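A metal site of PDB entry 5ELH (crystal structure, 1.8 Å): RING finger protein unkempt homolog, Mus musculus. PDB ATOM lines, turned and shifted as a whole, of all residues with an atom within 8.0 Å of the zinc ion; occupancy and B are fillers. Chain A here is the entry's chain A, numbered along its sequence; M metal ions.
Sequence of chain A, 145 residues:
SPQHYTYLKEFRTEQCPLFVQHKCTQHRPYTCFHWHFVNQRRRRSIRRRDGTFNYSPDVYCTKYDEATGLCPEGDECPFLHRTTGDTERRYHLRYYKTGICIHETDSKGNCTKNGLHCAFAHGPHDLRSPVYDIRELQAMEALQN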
ATOM      1  N   ARG A  12      -1.552  -1.227 -11.119  1.00  0.00           N
ATOM      2  CA  ARG A  12      -2.610  -2.236 -11.176  1.00  0.00           C
ATOM      3  C   ARG A  12      -2.363  -3.421 -10.265  1.00  0.00           C
ATOM      4  O   ARG A  12      -2.824  -4.530 -10.543  1.00  0.00           O
ATOM      5  CB  ARG A  12      -2.792  -2.722 -12.606  1.00  0.00           C
ATOM      6  CG  ARG A  12      -3.171  -1.625 -13.579  1.00  0.00           C
ATOM      7  CD  ARG A  12      -4.649  -1.363 -13.590  1.00  0.00           C
ATOM      8  NE  ARG A  12      -4.978  -0.345 -14.580  1.00  0.00           N
ATOM      9  CZ  ARG A  12      -4.982  -0.549 -15.896  1.00  0.00           C
ATOM     10  NH1 ARG A  12      -4.666  -1.743 -16.407  1.00  0.00           N
ATOM     11  NH2 ARG A  12      -5.292   0.440 -16.704  1.00  0.00           N
ATOM     12  N   GLU A  14      -3.030  -3.175  -6.802  1.00  0.00           N
ATOM     13  CA  GLU A  14      -3.972  -3.068  -5.683  1.00  0.00           C
ATOM     14  C   GLU A  14      -5.349  -2.654  -6.173  1.00  0.00           C
ATOM     15  O   GLU A  14      -5.471  -1.982  -7.203  1.00  0.00           O
ATOM     16  CB  GLU A  14      -3.478  -2.047  -4.657  1.00  0.00           C
ATOM     17  CG  GLU A  14      -2.125  -2.365  -4.027  1.00  0.00           C
ATOM     18  CD  GLU A  14      -2.173  -3.537  -3.080  1.00  0.00           C
ATOM     19  OE1 GLU A  14      -3.272  -3.831  -2.545  1.00  0.00           O
ATOM     20  OE2 GLU A  14      -1.118  -4.171  -2.874  1.00  0.00           O
ATOM     21  N   GLN A  15      -6.374  -3.022  -5.410  1.00  0.00           N
ATOM     22  CA  GLN A  15      -7.734  -2.700  -5.788  1.00  0.00           C
ATOM     23  C   GLN A  15      -8.044  -1.232  -5.557  1.00  0.00           C
ATOM     24  O   GLN A  15      -7.624  -0.642  -4.556  1.00  0.00           O
ATOM     25  CB  GLN A  15      -8.734  -3.540  -4.982  1.00  0.00           C
ATOM     26  CG  GLN A  15     -10.153  -3.402  -5.481  1.00  0.00           C
ATOM     27  CD  GLN A  15     -11.146  -4.215  -4.668  1.00  0.00           C
ATOM     28  OE1 GLN A  15     -10.966  -4.447  -3.477  1.00  0.00           O
ATOM     29  NE2 GLN A  15     -12.211  -4.652  -5.329  1.00  0.00           N
ATOM     30  N   CYS A  16      -8.793  -0.648  -6.482  1.00  0.00           N
ATOM     31  CA  CYS A  16      -9.215   0.747  -6.361  1.00  0.00           C
ATOM     32  C   CYS A  16     -10.297   0.883  -5.283  1.00  0.00           C
ATOM     33  O   CYS A  16     -11.397   0.343  -5.435  1.00  0.00           O
ATOM     34  CB  CYS A  16      -9.779   1.228  -7.710  1.00  0.00           C
ATOM     35  SG  CYS A  16     -10.366   2.951  -7.732  1.00  0.00           S
ATOM     36  N   PRO A  17      -9.997   1.620  -4.193  1.00  0.00           N
ATOM     37  CA  PRO A  17     -11.017   1.809  -3.144  1.00  0.00           C
ATOM     38  C   PRO A  17     -12.199   2.673  -3.589  1.00  0.00           C
ATOM     39  O   PRO A  17     -13.270   2.616  -2.976  1.00  0.00           O
ATOM     40  CB  PRO A  17     -10.239   2.497  -2.021  1.00  0.00           C
ATOM     41  CG  PRO A  17      -9.104   3.177  -2.706  1.00  0.00           C
ATOM     42  CD  PRO A  17      -8.726   2.277  -3.852  1.00  0.00           C
ATOM     43  N   LEU A  18     -12.019   3.478  -4.640  1.00  0.00           N
ATOM     44  CA  LEU A  18     -13.099   4.314  -5.139  1.00  0.00           C
ATOM     45  C   LEU A  18     -14.063   3.505  -6.009  1.00  0.00           C
ATOM     46  O   LEU A  18     -15.271   3.708  -5.958  1.00  0.00           O
ATOM     47  CB  LEU A  18     -12.558   5.499  -5.940  1.00  0.00           C
ATOM     48  CG  LEU A  18     -11.832   6.625  -5.179  1.00  0.00           C
ATOM     49  CD1 LEU A  18     -11.519   7.750  -6.151  1.00  0.00           C
ATOM     50  CD2 LEU A  18     -12.640   7.143  -4.004  1.00  0.00           C
ATOM     51  N   PHE A  19     -13.523   2.595  -6.820  1.00  0.00           N
ATOM     52  CA  PHE A  19     -14.340   1.859  -7.772  1.00  0.00           C
ATOM     53  C   PHE A  19     -15.394   1.006  -7.073  1.00  0.00           C
ATOM     54  O   PHE A  19     -16.542   0.900  -7.530  1.00  0.00           O
ATOM     55  CB  PHE A  19     -13.482   0.961  -8.671  1.00  0.00           C
ATOM     56  CG  PHE A  19     -14.300   0.093  -9.589  1.00  0.00           C
ATOM     57  CD1 PHE A  19     -14.920   0.636 -10.705  1.00  0.00           C
ATOM     58  CD2 PHE A  19     -14.493  -1.255  -9.299  1.00  0.00           C
ATOM     59  CE1 PHE A  19     -15.690  -0.158 -11.534  1.00  0.00           C
ATOM     60  CE2 PHE A  19     -15.253  -2.051 -10.129  1.00  0.00           C
ATOM     61  CZ  PHE A  19     -15.860  -1.497 -11.242  1.00  0.00           C
ATOM     62  N   VAL A  20     -15.006   0.408  -5.957  1.00  0.00           N
ATOM     63  CA  VAL A  20     -15.906  -0.464  -5.215  1.00  0.00           C
ATOM     64  C   VAL A  20     -17.125   0.306  -4.742  1.00  0.00           C
ATOM     65  O   VAL A  20     -18.156  -0.292  -4.410  1.00  0.00           O
ATOM     66  CB  VAL A  20     -15.192  -1.115  -4.007  1.00  0.00           C
ATOM     67  CG1 VAL A  20     -13.957  -1.879  -4.440  1.00  0.00           C
ATOM     68  CG2 VAL A  20     -14.775  -0.066  -3.001  1.00  0.00           C
ATOM     69  N   LYS A  23     -17.377   5.347  -7.180  1.00  0.00           N
ATOM     70  CA  LYS A  23     -16.890   6.713  -7.018  1.00  0.00           C
ATOM     71  C   LYS A  23     -15.632   6.962  -7.841  1.00  0.00           C
ATOM     72  O   LYS A  23     -15.101   8.069  -7.830  1.00  0.00           O
ATOM     73  CB  LYS A  23     -16.580   7.001  -5.538  1.00  0.00           C
ATOM     74  CG  LYS A  23     -17.787   7.079  -4.632  1.00  0.00           C
ATOM     75  CD  LYS A  23     -17.342   7.174  -3.174  1.00  0.00           C
ATOM     76  CE  LYS A  23     -18.516   7.320  -2.218  1.00  0.00           C
ATOM     77  NZ  LYS A  23     -18.073   7.304  -0.795  1.00  0.00           N
ATOM     78  N   CYS A  24     -15.141   5.941  -8.537  1.00  0.00           N
ATOM     79  CA  CYS A  24     -13.983   6.140  -9.403  1.00  0.00           C
ATOM     80  C   CYS A  24     -14.409   6.781 -10.728  1.00  0.00           C
ATOM     81  O   CYS A  24     -15.272   6.258 -11.424  1.00  0.00           O
ATOM     82  CB  CYS A  24     -13.224   4.851  -9.666  1.00  0.00           C
ATOM     83  SG  CYS A  24     -11.674   5.132 -10.571  1.00  0.00           S
ATOM     84  N   THR A  25     -13.795   7.922 -11.040  1.00  0.00           N
ATOM     85  CA  THR A  25     -14.083   8.661 -12.262  1.00  0.00           C
ATOM     86  C   THR A  25     -13.185   8.236 -13.403  1.00  0.00           C
ATOM     87  O   THR A  25     -13.253   8.817 -14.490  1.00  0.00           O
ATOM     88  CB  THR A  25     -13.836  10.168 -12.062  1.00  0.00           C
ATOM     89  OG1 THR A  25     -12.439  10.402 -11.864  1.00  0.00           O
ATOM     90  CG2 THR A  25     -14.613  10.679 -10.867  1.00  0.00           C
ATOM     91  N   GLN A  26     -12.321   7.251 -13.146  1.00  0.00           N
ATOM     92  CA  GLN A  26     -11.331   6.806 -14.124  1.00  0.00           C
ATOM     93  C   GLN A  26     -11.600   5.385 -14.594  1.00  0.00           C
ATOM     94  O   GLN A  26     -10.673   4.592 -14.782  1.00  0.00           O
ATOM     95  CB  GLN A  26      -9.925   6.902 -13.525  1.00  0.00           C
ATOM     96  CG  GLN A  26      -9.455   8.327 -13.263  1.00  0.00           C
ATOM     97  CD  GLN A  26      -8.090   8.371 -12.628  1.00  0.00           C
ATOM     98  OE1 GLN A  26      -7.712   7.463 -11.878  1.00  0.00           O
ATOM     99  NE2 GLN A  26      -7.331   9.424 -12.916  1.00  0.00           N
ATOM    100  N   HIS A  27     -12.883   5.066 -14.774  1.00  0.00           N
ATOM    101  CA  HIS A  27     -13.317   3.800 -15.343  1.00  0.00           C
ATOM    102  C   HIS A  27     -14.041   4.093 -16.651  1.00  0.00           C
ATOM    103  O   HIS A  27     -15.097   4.728 -16.627  1.00  0.00           O
ATOM    104  CB  HIS A  27     -14.279   3.095 -14.386  1.00  0.00           C
ATOM    105  CG  HIS A  27     -14.887   1.837 -14.944  1.00  0.00           C
ATOM    106  ND1 HIS A  27     -14.249   0.615 -14.904  1.00  0.00           N
ATOM    107  CD2 HIS A  27     -16.060   1.614 -15.576  1.00  0.00           C
ATOM    108  CE1 HIS A  27     -15.006  -0.300 -15.468  1.00  0.00           C
ATOM    109  NE2 HIS A  27     -16.115   0.284 -15.887  1.00  0.00           N
ATOM    110  N   TYR A  30     -10.849   3.788 -18.951  1.00  0.00           N
ATOM    111  CA  TYR A  30     -10.199   3.188 -17.801  1.00  0.00           C
ATOM    112  C   TYR A  30      -8.754   3.670 -17.685  1.00  0.00           C
ATOM    113  O   TYR A  30      -7.844   3.039 -18.194  1.00  0.00           O
ATOM    114  CB  TYR A  30     -10.259   1.659 -17.929  1.00  0.00           C
ATOM    115  CG  TYR A  30      -9.609   0.902 -16.790  1.00  0.00           C
ATOM    116  CD1 TYR A  30      -9.845   1.255 -15.462  1.00  0.00           C
ATOM    117  CD2 TYR A  30      -8.786  -0.187 -17.044  1.00  0.00           C
ATOM    118  CE1 TYR A  30      -9.265   0.548 -14.425  1.00  0.00           C
ATOM    119  CE2 TYR A  30      -8.194  -0.888 -16.012  1.00  0.00           C
ATOM    120  CZ  TYR A  30      -8.430  -0.526 -14.712  1.00  0.00           C
ATOM    121  OH  TYR A  30      -7.832  -1.238 -13.699  1.00  0.00           O
ATOM    122  N   THR A  31      -8.562   4.810 -17.019  1.00  0.00           N
ATOM    123  CA  THR A  31      -7.224   5.378 -16.831  1.00  0.00           C
ATOM    124  C   THR A  31      -6.724   5.184 -15.409  1.00  0.00           C
ATOM    125  O   THR A  31      -5.744   5.813 -15.001  1.00  0.00           O
ATOM    126  CB  THR A  31      -7.215   6.885 -17.093  1.00  0.00           C
ATOM    127  OG1 THR A  31      -8.000   7.547 -16.089  1.00  0.00           O
ATOM    128  CG2 THR A  31      -7.762   7.203 -18.477  1.00  0.00           C
ATOM    129  N   CYS A  32      -7.397   4.337 -14.639  1.00  0.00           N
ATOM    130  CA  CYS A  32      -7.064   4.219 -13.230  1.00  0.00           C
ATOM    131  C   CYS A  32      -5.758   3.478 -13.037  1.00  0.00           C
ATOM    132  O   CYS A  32      -5.410   2.569 -13.794  1.00  0.00           O
ATOM    133  CB  CYS A  32      -8.171   3.527 -12.431  1.00  0.00           C
ATOM    134  SG  CYS A  32      -7.962   3.717 -10.626  1.00  0.00           S
ATOM    135  N   PHE A  33      -5.032   3.880 -12.008  1.00  0.00           N
ATOM    136  CA  PHE A  33      -3.762   3.265 -11.666  1.00  0.00           C
ATOM    137  C   PHE A  33      -3.966   1.930 -10.943  1.00  0.00           C
ATOM    138  O   PHE A  33      -3.054   1.106 -10.860  1.00  0.00           O
ATOM    139  CB  PHE A  33      -2.976   4.219 -10.773  1.00  0.00           C
ATOM    140  CG  PHE A  33      -1.541   3.876 -10.654  1.00  0.00           C
ATOM    141  CD1 PHE A  33      -0.646   4.259 -11.647  1.00  0.00           C
ATOM    142  CD2 PHE A  33      -1.064   3.156  -9.575  1.00  0.00           C
ATOM    143  CE1 PHE A  33       0.689   3.936 -11.550  1.00  0.00           C
ATOM    144  CE2 PHE A  33       0.264   2.841  -9.468  1.00  0.00           C
ATOM    145  CZ  PHE A  33       1.137   3.220 -10.456  1.00  0.00           C
ATOM    146  N   HIS A  34      -5.171   1.713 -10.436  1.00  0.00           N
ATOM    147  CA  HIS A  34      -5.479   0.542  -9.626  1.00  0.00           C
ATOM    148  C   HIS A  34      -6.395  -0.400 -10.381  1.00  0.00           C
ATOM    149  O   HIS A  34      -7.018   0.011 -11.359  1.00  0.00           O
ATOM    150  CB  HIS A  34      -6.134   1.012  -8.334  1.00  0.00           C
ATOM    151  CG  HIS A  34      -5.319   2.007  -7.584  1.00  0.00           C
ATOM    152  ND1 HIS A  34      -4.086   1.694  -7.033  1.00  0.00           N
ATOM    153  CD2 HIS A  34      -5.522   3.320  -7.320  1.00  0.00           C
ATOM    154  CE1 HIS A  34      -3.587   2.768  -6.448  1.00  0.00           C
ATOM    155  NE2 HIS A  34      -4.439   3.768  -6.612  1.00  0.00           N
ATOM    156  N   TRP A  35      -6.482  -1.659  -9.976  1.00  0.00           N
ATOM    157  CA  TRP A  35      -7.377  -2.581 -10.666  1.00  0.00           C
ATOM    158  C   TRP A  35      -8.805  -2.417 -10.168  1.00  0.00           C
ATOM    159  O   TRP A  35      -9.053  -2.094  -9.005  1.00  0.00           O
ATOM    160  CB  TRP A  35      -6.907  -4.046 -10.624  1.00  0.00           C
ATOM    161  CG  TRP A  35      -6.803  -4.732  -9.296  1.00  0.00           C
ATOM    162  CD1 TRP A  35      -5.690  -4.929  -8.561  1.00  0.00           C
ATOM    163  CD2 TRP A  35      -7.875  -5.377  -8.586  1.00  0.00           C
ATOM    164  NE1 TRP A  35      -5.982  -5.636  -7.420  1.00  0.00           N
ATOM    165  CE2 TRP A  35      -7.323  -5.923  -7.419  1.00  0.00           C
ATOM    166  CE3 TRP A  35      -9.242  -5.524  -8.824  1.00  0.00           C
ATOM    167  CZ2 TRP A  35      -8.087  -6.619  -6.477  1.00  0.00           C
ATOM    168  CZ3 TRP A  35     -10.013  -6.209  -7.886  1.00  0.00           C
ATOM    169  CH2 TRP A  35      -9.419  -6.748  -6.732  1.00  0.00           C
ATOM    170  N   HIS A  36      -9.739  -2.621 -11.092  1.00  0.00           N
ATOM    171  CA  HIS A  36     -11.162  -2.531 -10.785  1.00  0.00           C
ATOM    172  C   HIS A  36     -11.759  -3.943 -10.762  1.00  0.00           C
ATOM    173  O   HIS A  36     -12.548  -4.284  -9.882  1.00  0.00           O
ATOM    174  CB  HIS A  36     -11.869  -1.639 -11.810  1.00  0.00           C
ATOM    175  CG  HIS A  36     -11.566  -0.176 -11.668  1.00  0.00           C
ATOM    176  ND1 HIS A  36     -12.183   0.778 -12.445  1.00  0.00           N
ATOM    177  CD2 HIS A  36     -10.719   0.486 -10.856  1.00  0.00           C
ATOM    178  CE1 HIS A  36     -11.725   1.977 -12.111  1.00  0.00           C
ATOM    179  NE2 HIS A  36     -10.847   1.833 -11.143  1.00  0.00           N
ATOM    180  N   GLN A  40      -7.953  -7.675 -14.026  1.00  0.00           N
ATOM    181  CA  GLN A  40      -7.048  -6.564 -14.365  1.00  0.00           C
ATOM    182  C   GLN A  40      -5.822  -6.506 -13.465  1.00  0.00           C
ATOM    183  O   GLN A  40      -4.866  -5.771 -13.748  1.00  0.00           O
ATOM    184  CB  GLN A  40      -7.784  -5.243 -14.285  1.00  0.00           C
ATOM    185  CG  GLN A  40      -8.946  -5.125 -15.221  1.00  0.00           C
ATOM    186  CD  GLN A  40      -9.795  -3.909 -14.935  1.00  0.00           C
ATOM    187  OE1 GLN A  40     -10.049  -3.571 -13.767  1.00  0.00           O
ATOM    188  NE2 GLN A  40     -10.240  -3.237 -15.984  1.00  0.00           N
HETATM  189 ZN    ZN M   1     -10.212   3.388  -9.987  1.00  0.00          ZN
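Four residues have an atom within 4 Å of the zinc ion: Cys 16, Cys 24, Cys 32 and His 36.
ND1 of His 27 is in hydrogen-bond range of ND1 of His 36 (3.2 Å). The backbone NH (N) of His 36 is in hydrogen-bond range of the side-chain amide oxygen (OE1) of Gln 40, 2.9 Å away. The side-chain sulfur (SG) of Cys 16 sits close to the backbone NH (N) of Phe 19, 3.3 Å away. The side-chain sulfur of Cys 16 sits close to the backbone NH of Leu 18, 3.5 Å away. The backbone NH (N) of Cys 16 is in hydrogen-bond range of the backbone carbonyl oxygen (O) of Trp 35 (2.9 Å). The backbone NH (N) of Cys 24 lies within hydrogen-bond range of the backbone carbonyl oxygen (O) of Leu 18 (3.4 Å). SG of Cys 32 sits close to N of His 34, 3.4 Å away. The guanidinium group (NE) of Arg 12 lies within hydrogen-bond range of the backbone carbonyl oxygen (O) of Cys 32 (3.0 Å).
The zinc ion is bound by a ring nitrogen (NE2) of His 36 (2.0 Å). SG of Cys 16 binds the zinc ion (2.3 Å). SG of Cys 24 is bound to the zinc ion (2.3 Å). The zinc ion is bound by SG of Cys 32 (2.4 Å). The zinc ion has four donor atoms within binding distance.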
